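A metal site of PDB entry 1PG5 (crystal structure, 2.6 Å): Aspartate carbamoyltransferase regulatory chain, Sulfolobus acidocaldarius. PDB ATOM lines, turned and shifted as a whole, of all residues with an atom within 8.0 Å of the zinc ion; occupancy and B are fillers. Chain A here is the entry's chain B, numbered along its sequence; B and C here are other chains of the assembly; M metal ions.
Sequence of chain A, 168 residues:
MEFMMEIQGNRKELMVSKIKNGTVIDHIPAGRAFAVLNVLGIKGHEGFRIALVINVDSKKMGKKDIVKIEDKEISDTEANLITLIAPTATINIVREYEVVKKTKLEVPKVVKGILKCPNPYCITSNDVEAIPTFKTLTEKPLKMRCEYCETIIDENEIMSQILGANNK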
ATOM      1  N   LYS A 116     -20.816  -9.053  23.521  1.00  0.00           N
ATOM      2  CA  LYS A 116     -20.684 -10.463  23.757  1.00  0.00           C
ATOM      3  C   LYS A 116     -21.702 -11.033  24.700  1.00  0.00           C
ATOM      4  O   LYS A 116     -22.225 -10.374  25.555  1.00  0.00           O
ATOM      5  CB  LYS A 116     -19.297 -10.761  24.285  1.00  0.00           C
ATOM      6  CG  LYS A 116     -18.176 -10.339  23.313  1.00  0.00           C
ATOM      7  CD  LYS A 116     -16.810 -10.923  23.745  1.00  0.00           C
ATOM      8  CE  LYS A 116     -15.632 -10.382  22.963  1.00  0.00           C
ATOM      9  NZ  LYS A 116     -14.376 -10.823  23.644  1.00  0.00           N
ATOM     10  N   CYS A 117     -21.951 -12.303  24.568  1.00  0.00           N
ATOM     11  CA  CYS A 117     -22.862 -12.986  25.493  1.00  0.00           C
ATOM     12  C   CYS A 117     -22.062 -13.556  26.668  1.00  0.00           C
ATOM     13  O   CYS A 117     -21.050 -14.265  26.512  1.00  0.00           O
ATOM     14  CB  CYS A 117     -23.588 -14.103  24.748  1.00  0.00           C
ATOM     15  SG  CYS A 117     -24.897 -14.963  25.597  1.00  0.00           S
ATOM     16  N   PRO A 118     -22.518 -13.210  27.855  1.00  0.00           N
ATOM     17  CA  PRO A 118     -21.835 -13.652  29.078  1.00  0.00           C
ATOM     18  C   PRO A 118     -21.980 -15.144  29.415  1.00  0.00           C
ATOM     19  O   PRO A 118     -21.395 -15.609  30.355  1.00  0.00           O
ATOM     20  CB  PRO A 118     -22.453 -12.752  30.162  1.00  0.00           C
ATOM     21  CG  PRO A 118     -23.785 -12.288  29.586  1.00  0.00           C
ATOM     22  CD  PRO A 118     -23.669 -12.309  28.119  1.00  0.00           C
ATOM     23  N   ASN A 119     -22.783 -15.872  28.650  1.00  0.00           N
ATOM     24  CA  ASN A 119     -22.938 -17.304  28.843  1.00  0.00           C
ATOM     25  C   ASN A 119     -21.803 -18.027  28.095  1.00  0.00           C
ATOM     26  O   ASN A 119     -21.689 -17.997  26.903  1.00  0.00           O
ATOM     27  CB  ASN A 119     -24.364 -17.725  28.487  1.00  0.00           C
ATOM     28  CG  ASN A 119     -24.496 -19.210  28.272  1.00  0.00           C
ATOM     29  OD1 ASN A 119     -23.736 -20.020  28.771  1.00  0.00           O
ATOM     30  ND2 ASN A 119     -25.443 -19.571  27.467  1.00  0.00           N
ATOM     31  N   PRO A 120     -20.876 -18.630  28.840  1.00  0.00           N
ATOM     32  CA  PRO A 120     -19.733 -19.275  28.177  1.00  0.00           C
ATOM     33  C   PRO A 120     -20.144 -20.485  27.376  1.00  0.00           C
ATOM     34  O   PRO A 120     -19.324 -20.999  26.645  1.00  0.00           O
ATOM     35  CB  PRO A 120     -18.833 -19.680  29.335  1.00  0.00           C
ATOM     36  CG  PRO A 120     -19.847 -19.890  30.507  1.00  0.00           C
ATOM     37  CD  PRO A 120     -20.792 -18.710  30.329  1.00  0.00           C
ATOM     38  N   TYR A 121     -21.375 -20.970  27.521  1.00  0.00           N
ATOM     39  CA  TYR A 121     -21.840 -22.144  26.762  1.00  0.00           C
ATOM     40  C   TYR A 121     -22.716 -21.726  25.607  1.00  0.00           C
ATOM     41  O   TYR A 121     -23.304 -22.554  24.971  1.00  0.00           O
ATOM     42  CB  TYR A 121     -22.622 -23.108  27.655  1.00  0.00           C
ATOM     43  CG  TYR A 121     -21.747 -23.810  28.659  1.00  0.00           C
ATOM     44  CD1 TYR A 121     -21.725 -23.395  29.987  1.00  0.00           C
ATOM     45  CD2 TYR A 121     -20.962 -24.927  28.295  1.00  0.00           C
ATOM     46  CE1 TYR A 121     -20.962 -24.037  30.913  1.00  0.00           C
ATOM     47  CE2 TYR A 121     -20.183 -25.585  29.228  1.00  0.00           C
ATOM     48  CZ  TYR A 121     -20.183 -25.078  30.541  1.00  0.00           C
ATOM     49  OH  TYR A 121     -19.446 -25.647  31.515  1.00  0.00           O
ATOM     50  N   CYS A 122     -22.777 -20.443  25.292  1.00  0.00           N
ATOM     51  CA  CYS A 122     -23.531 -19.995  24.123  1.00  0.00           C
ATOM     52  C   CYS A 122     -22.675 -20.238  22.942  1.00  0.00           C
ATOM     53  O   CYS A 122     -21.493 -19.951  23.048  1.00  0.00           O
ATOM     54  CB  CYS A 122     -23.805 -18.500  24.271  1.00  0.00           C
ATOM     55  SG  CYS A 122     -24.699 -17.731  22.917  1.00  0.00           S
ATOM     56  N   ILE A 123     -23.232 -20.751  21.843  1.00  0.00           N
ATOM     57  CA  ILE A 123     -22.513 -20.915  20.598  1.00  0.00           C
ATOM     58  C   ILE A 123     -21.751 -19.651  20.170  1.00  0.00           C
ATOM     59  O   ILE A 123     -20.634 -19.791  19.698  1.00  0.00           O
ATOM     60  CB  ILE A 123     -23.440 -21.360  19.503  1.00  0.00           C
ATOM     61  CG1 ILE A 123     -22.648 -21.928  18.312  1.00  0.00           C
ATOM     62  CG2 ILE A 123     -24.432 -20.236  19.104  1.00  0.00           C
ATOM     63  CD1 ILE A 123     -21.814 -23.143  18.682  1.00  0.00           C
ATOM     64  N   THR A 124     -22.296 -18.448  20.395  1.00  0.00           N
ATOM     65  CA  THR A 124     -21.568 -17.187  20.100  1.00  0.00           C
ATOM     66  C   THR A 124     -20.276 -16.909  20.914  1.00  0.00           C
ATOM     67  O   THR A 124     -19.425 -16.119  20.500  1.00  0.00           O
ATOM     68  CB  THR A 124     -22.511 -15.987  20.165  1.00  0.00           C
ATOM     69  OG1 THR A 124     -23.032 -15.772  21.487  1.00  0.00           O
ATOM     70  CG2 THR A 124     -23.780 -16.354  19.338  1.00  0.00           C
ATOM     71  N   SER A 125     -20.138 -17.593  22.042  1.00  0.00           N
ATOM     72  CA  SER A 125     -18.970 -17.462  22.937  1.00  0.00           C
ATOM     73  C   SER A 125     -17.992 -18.534  22.551  1.00  0.00           C
ATOM     74  O   SER A 125     -17.002 -18.614  23.171  1.00  0.00           O
ATOM     75  CB  SER A 125     -19.348 -17.677  24.401  1.00  0.00           C
ATOM     76  OG  SER A 125     -20.226 -16.649  24.894  1.00  0.00           O
ATOM     77  N   PRO A 132     -22.170 -12.770  17.921  1.00  0.00           N
ATOM     78  CA  PRO A 132     -23.123 -12.377  18.954  1.00  0.00           C
ATOM     79  C   PRO A 132     -24.209 -11.398  18.483  1.00  0.00           C
ATOM     80  O   PRO A 132     -23.846 -10.442  17.869  1.00  0.00           O
ATOM     81  CB  PRO A 132     -22.222 -11.682  19.984  1.00  0.00           C
ATOM     82  CG  PRO A 132     -20.827 -12.222  19.746  1.00  0.00           C
ATOM     83  CD  PRO A 132     -20.779 -12.611  18.381  1.00  0.00           C
ATOM     84  N   THR A 133     -25.469 -11.684  18.806  1.00  0.00           N
ATOM     85  CA  THR A 133     -26.615 -10.900  18.422  1.00  0.00           C
ATOM     86  C   THR A 133     -27.593 -10.810  19.607  1.00  0.00           C
ATOM     87  O   THR A 133     -28.035 -11.847  20.139  1.00  0.00           O
ATOM     88  CB  THR A 133     -27.269 -11.651  17.271  1.00  0.00           C
ATOM     89  OG1 THR A 133     -26.308 -11.816  16.257  1.00  0.00           O
ATOM     90  CG2 THR A 133     -28.358 -10.864  16.577  1.00  0.00           C
ATOM     91  N   PHE A 134     -27.935  -9.577  19.964  1.00  0.00           N
ATOM     92  CA  PHE A 134     -28.911  -9.219  21.016  1.00  0.00           C
ATOM     93  C   PHE A 134     -30.078  -8.467  20.422  1.00  0.00           C
ATOM     94  O   PHE A 134     -29.890  -7.545  19.641  1.00  0.00           O
ATOM     95  CB  PHE A 134     -28.177  -8.422  22.089  1.00  0.00           C
ATOM     96  CG  PHE A 134     -27.404  -9.318  23.015  1.00  0.00           C
ATOM     97  CD1 PHE A 134     -26.124  -9.797  22.649  1.00  0.00           C
ATOM     98  CD2 PHE A 134     -28.010  -9.813  24.175  1.00  0.00           C
ATOM     99  CE1 PHE A 134     -25.449 -10.671  23.473  1.00  0.00           C
ATOM    100  CE2 PHE A 134     -27.297 -10.693  25.064  1.00  0.00           C
ATOM    101  CZ  PHE A 134     -26.044 -11.108  24.710  1.00  0.00           C
ATOM    102  N   ARG A 145     -31.687  -9.327  24.879  1.00  0.00           N
ATOM    103  CA  ARG A 145     -31.623 -10.764  24.968  1.00  0.00           C
ATOM    104  C   ARG A 145     -30.877 -11.394  23.848  1.00  0.00           C
ATOM    105  O   ARG A 145     -31.218 -11.107  22.713  1.00  0.00           O
ATOM    106  CB  ARG A 145     -33.005 -11.275  24.806  1.00  0.00           C
ATOM    107  CG  ARG A 145     -33.259 -12.489  25.595  1.00  0.00           C
ATOM    108  CD  ARG A 145     -34.080 -13.445  24.895  1.00  0.00           C
ATOM    109  NE  ARG A 145     -35.504 -13.164  24.890  1.00  0.00           N
ATOM    110  CZ  ARG A 145     -36.217 -12.935  23.790  1.00  0.00           C
ATOM    111  NH1 ARG A 145     -37.535 -12.778  23.928  1.00  0.00           N
ATOM    112  NH2 ARG A 145     -35.610 -12.854  22.574  1.00  0.00           N
ATOM    113  N   CYS A 146     -29.942 -12.317  24.169  1.00  0.00           N
ATOM    114  CA  CYS A 146     -29.274 -13.175  23.176  1.00  0.00           C
ATOM    115  C   CYS A 146     -30.221 -14.028  22.330  1.00  0.00           C
ATOM    116  O   CYS A 146     -31.098 -14.736  22.827  1.00  0.00           O
ATOM    117  CB  CYS A 146     -28.283 -14.070  23.892  1.00  0.00           C
ATOM    118  SG  CYS A 146     -27.219 -15.140  22.884  1.00  0.00           S
ATOM    119  N   GLU A 147     -30.122 -13.888  21.032  1.00  0.00           N
ATOM    120  CA  GLU A 147     -30.954 -14.644  20.114  1.00  0.00           C
ATOM    121  C   GLU A 147     -30.628 -16.127  20.026  1.00  0.00           C
ATOM    122  O   GLU A 147     -31.448 -16.895  19.591  1.00  0.00           O
ATOM    123  CB  GLU A 147     -30.860 -14.029  18.749  1.00  0.00           C
ATOM    124  CG  GLU A 147     -31.497 -12.595  18.663  1.00  0.00           C
ATOM    125  CD  GLU A 147     -31.531 -12.118  17.195  1.00  0.00           C
ATOM    126  OE1 GLU A 147     -31.281 -13.019  16.321  1.00  0.00           O
ATOM    127  OE2 GLU A 147     -31.791 -10.917  16.907  1.00  0.00           O
ATOM    128  N   TYR A 148     -29.455 -16.542  20.499  1.00  0.00           N
ATOM    129  CA  TYR A 148     -29.108 -17.942  20.512  1.00  0.00           C
ATOM    130  C   TYR A 148     -29.501 -18.671  21.782  1.00  0.00           C
ATOM    131  O   TYR A 148     -30.042 -19.758  21.738  1.00  0.00           O
ATOM    132  CB  TYR A 148     -27.610 -18.011  20.254  1.00  0.00           C
ATOM    133  CG  TYR A 148     -27.368 -17.589  18.866  1.00  0.00           C
ATOM    134  CD1 TYR A 148     -27.507 -18.508  17.802  1.00  0.00           C
ATOM    135  CD2 TYR A 148     -27.087 -16.276  18.562  1.00  0.00           C
ATOM    136  CE1 TYR A 148     -27.261 -18.121  16.475  1.00  0.00           C
ATOM    137  CE2 TYR A 148     -26.872 -15.870  17.199  1.00  0.00           C
ATOM    138  CZ  TYR A 148     -26.984 -16.801  16.186  1.00  0.00           C
ATOM    139  OH  TYR A 148     -26.797 -16.412  14.877  1.00  0.00           O
ATOM    140  N   CYS A 149     -29.240 -18.053  22.918  1.00  0.00           N
ATOM    141  CA  CYS A 149     -29.461 -18.674  24.227  1.00  0.00           C
ATOM    142  C   CYS A 149     -30.400 -17.965  25.182  1.00  0.00           C
ATOM    143  O   CYS A 149     -30.605 -18.451  26.261  1.00  0.00           O
ATOM    144  CB  CYS A 149     -28.104 -18.861  24.913  1.00  0.00           C
ATOM    145  SG  CYS A 149     -27.377 -17.391  25.601  1.00  0.00           S
ATOM    146  N   GLU A 150     -30.965 -16.826  24.825  1.00  0.00           N
ATOM    147  CA  GLU A 150     -31.952 -16.147  25.682  1.00  0.00           C
ATOM    148  C   GLU A 150     -31.379 -15.524  26.968  1.00  0.00           C
ATOM    149  O   GLU A 150     -32.137 -15.007  27.794  1.00  0.00           O
ATOM    150  CB  GLU A 150     -33.171 -16.998  26.010  1.00  0.00           C
ATOM    151  CG  GLU A 150     -33.931 -17.714  24.865  1.00  0.00           C
ATOM    152  CD  GLU A 150     -33.932 -17.122  23.437  1.00  0.00           C
ATOM    153  OE1 GLU A 150     -33.645 -17.933  22.530  1.00  0.00           O
ATOM    154  OE2 GLU A 150     -34.300 -15.932  23.172  1.00  0.00           O
ATOM    155  N   THR A 151     -30.051 -15.469  27.118  1.00  0.00           N
ATOM    156  CA  THR A 151     -29.489 -14.751  28.248  1.00  0.00           C
ATOM    157  C   THR A 151     -29.799 -13.283  28.143  1.00  0.00           C
ATOM    158  O   THR A 151     -29.686 -12.709  27.067  1.00  0.00           O
ATOM    159  CB  THR A 151     -27.993 -14.974  28.283  1.00  0.00           C
ATOM    160  OG1 THR A 151     -27.737 -16.324  28.757  1.00  0.00           O
ATOM    161  CG2 THR A 151     -27.318 -14.093  29.346  1.00  0.00           C
ATOM    162  N   ILE A 152     -30.179 -12.667  29.257  1.00  0.00           N
ATOM    163  CA  ILE A 152     -30.562 -11.276  29.264  1.00  0.00           C
ATOM    164  C   ILE A 152     -29.414 -10.400  29.773  1.00  0.00           C
ATOM    165  O   ILE A 152     -28.753 -10.790  30.679  1.00  0.00           O
ATOM    166  CB  ILE A 152     -31.801 -11.097  30.096  1.00  0.00           C
ATOM    167  CG1 ILE A 152     -32.976 -11.690  29.326  1.00  0.00           C
ATOM    168  CG2 ILE A 152     -32.025  -9.620  30.408  1.00  0.00           C
ATOM    169  CD1 ILE A 152     -34.286 -11.586  30.042  1.00  0.00           C
ATOM    170  N   ASP B 105     -25.526 -23.863  23.780  1.00  0.00           N
ATOM    171  CA  ASP B 105     -26.857 -23.274  23.556  1.00  0.00           C
ATOM    172  C   ASP B 105     -26.856 -22.518  22.241  1.00  0.00           C
ATOM    173  O   ASP B 105     -25.967 -21.752  21.991  1.00  0.00           O
ATOM    174  CB  ASP B 105     -27.166 -22.249  24.658  1.00  0.00           C
ATOM    175  CG  ASP B 105     -27.093 -22.836  26.054  1.00  0.00           C
ATOM    176  OD1 ASP B 105     -27.831 -23.771  26.283  1.00  0.00           O
ATOM    177  OD2 ASP B 105     -26.322 -22.460  26.966  1.00  0.00           O
ATOM    178  N   GLY B 106     -27.852 -22.733  21.411  1.00  0.00           N
ATOM    179  CA  GLY B 106     -27.986 -21.919  20.209  1.00  0.00           C
ATOM    180  C   GLY B 106     -27.285 -22.582  19.070  1.00  0.00           C
ATOM    181  O   GLY B 106     -27.328 -22.087  17.959  1.00  0.00           O
ATOM    182  N   MET C 231     -21.926 -18.203  35.576  1.00  0.00           N
ATOM    183  CA  MET C 231     -22.506 -16.846  35.393  1.00  0.00           C
ATOM    184  C   MET C 231     -22.955 -16.025  36.635  1.00  0.00           C
ATOM    185  O   MET C 231     -23.020 -14.793  36.578  1.00  0.00           O
ATOM    186  CB  MET C 231     -23.717 -16.916  34.444  1.00  0.00           C
ATOM    187  CG  MET C 231     -23.383 -16.926  32.974  1.00  0.00           C
ATOM    188  SD  MET C 231     -24.842 -17.155  31.973  1.00  0.00           S
ATOM    189  CE  MET C 231     -25.666 -15.551  32.133  1.00  0.00           C
HETATM  190 ZN    ZN M   1     -25.979 -16.306  24.235  1.00  0.00          ZN
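Four residues have an atom within 4 Å of the zinc ion: Cys 117, Cys 122, Cys 146 and Cys 149. The nearest printed residue that does not touch the zinc ion is Thr 124 (4.1 Å).
The zinc ion is bound by the side-chain sulfur (SG) of Cys 146 (2.2 Å), the side-chain sulfur (SG) of Cys 117 (2.2 Å), the side-chain sulfur (SG) of Cys 149 (2.2 Å) and the side-chain sulfur (SG) of Cys 122 (2.3 Å). The zinc ion has four donor atoms within binding distance.
SG of Cys 122 sits close to OG1 of Thr 124 (2.9 Å). O of Thr 151 lies within hydrogen-bond range of N of Cys 146 (2.9 Å). The side-chain sulfur (SG) of Cys 146 lies close to the backbone NH (N) of Tyr 148, 3.6 Å away. OG of Ser 125 sits at hydrogen-bond distance from O of Cys 117 (3.0 Å). The side-chain hydroxyl of Thr 151 lies close to the side-chain sulfur of Cys 149 (3.4 Å). ND2 of Asn 119 lies close to SG of Cys 149, 3.5 Å away.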
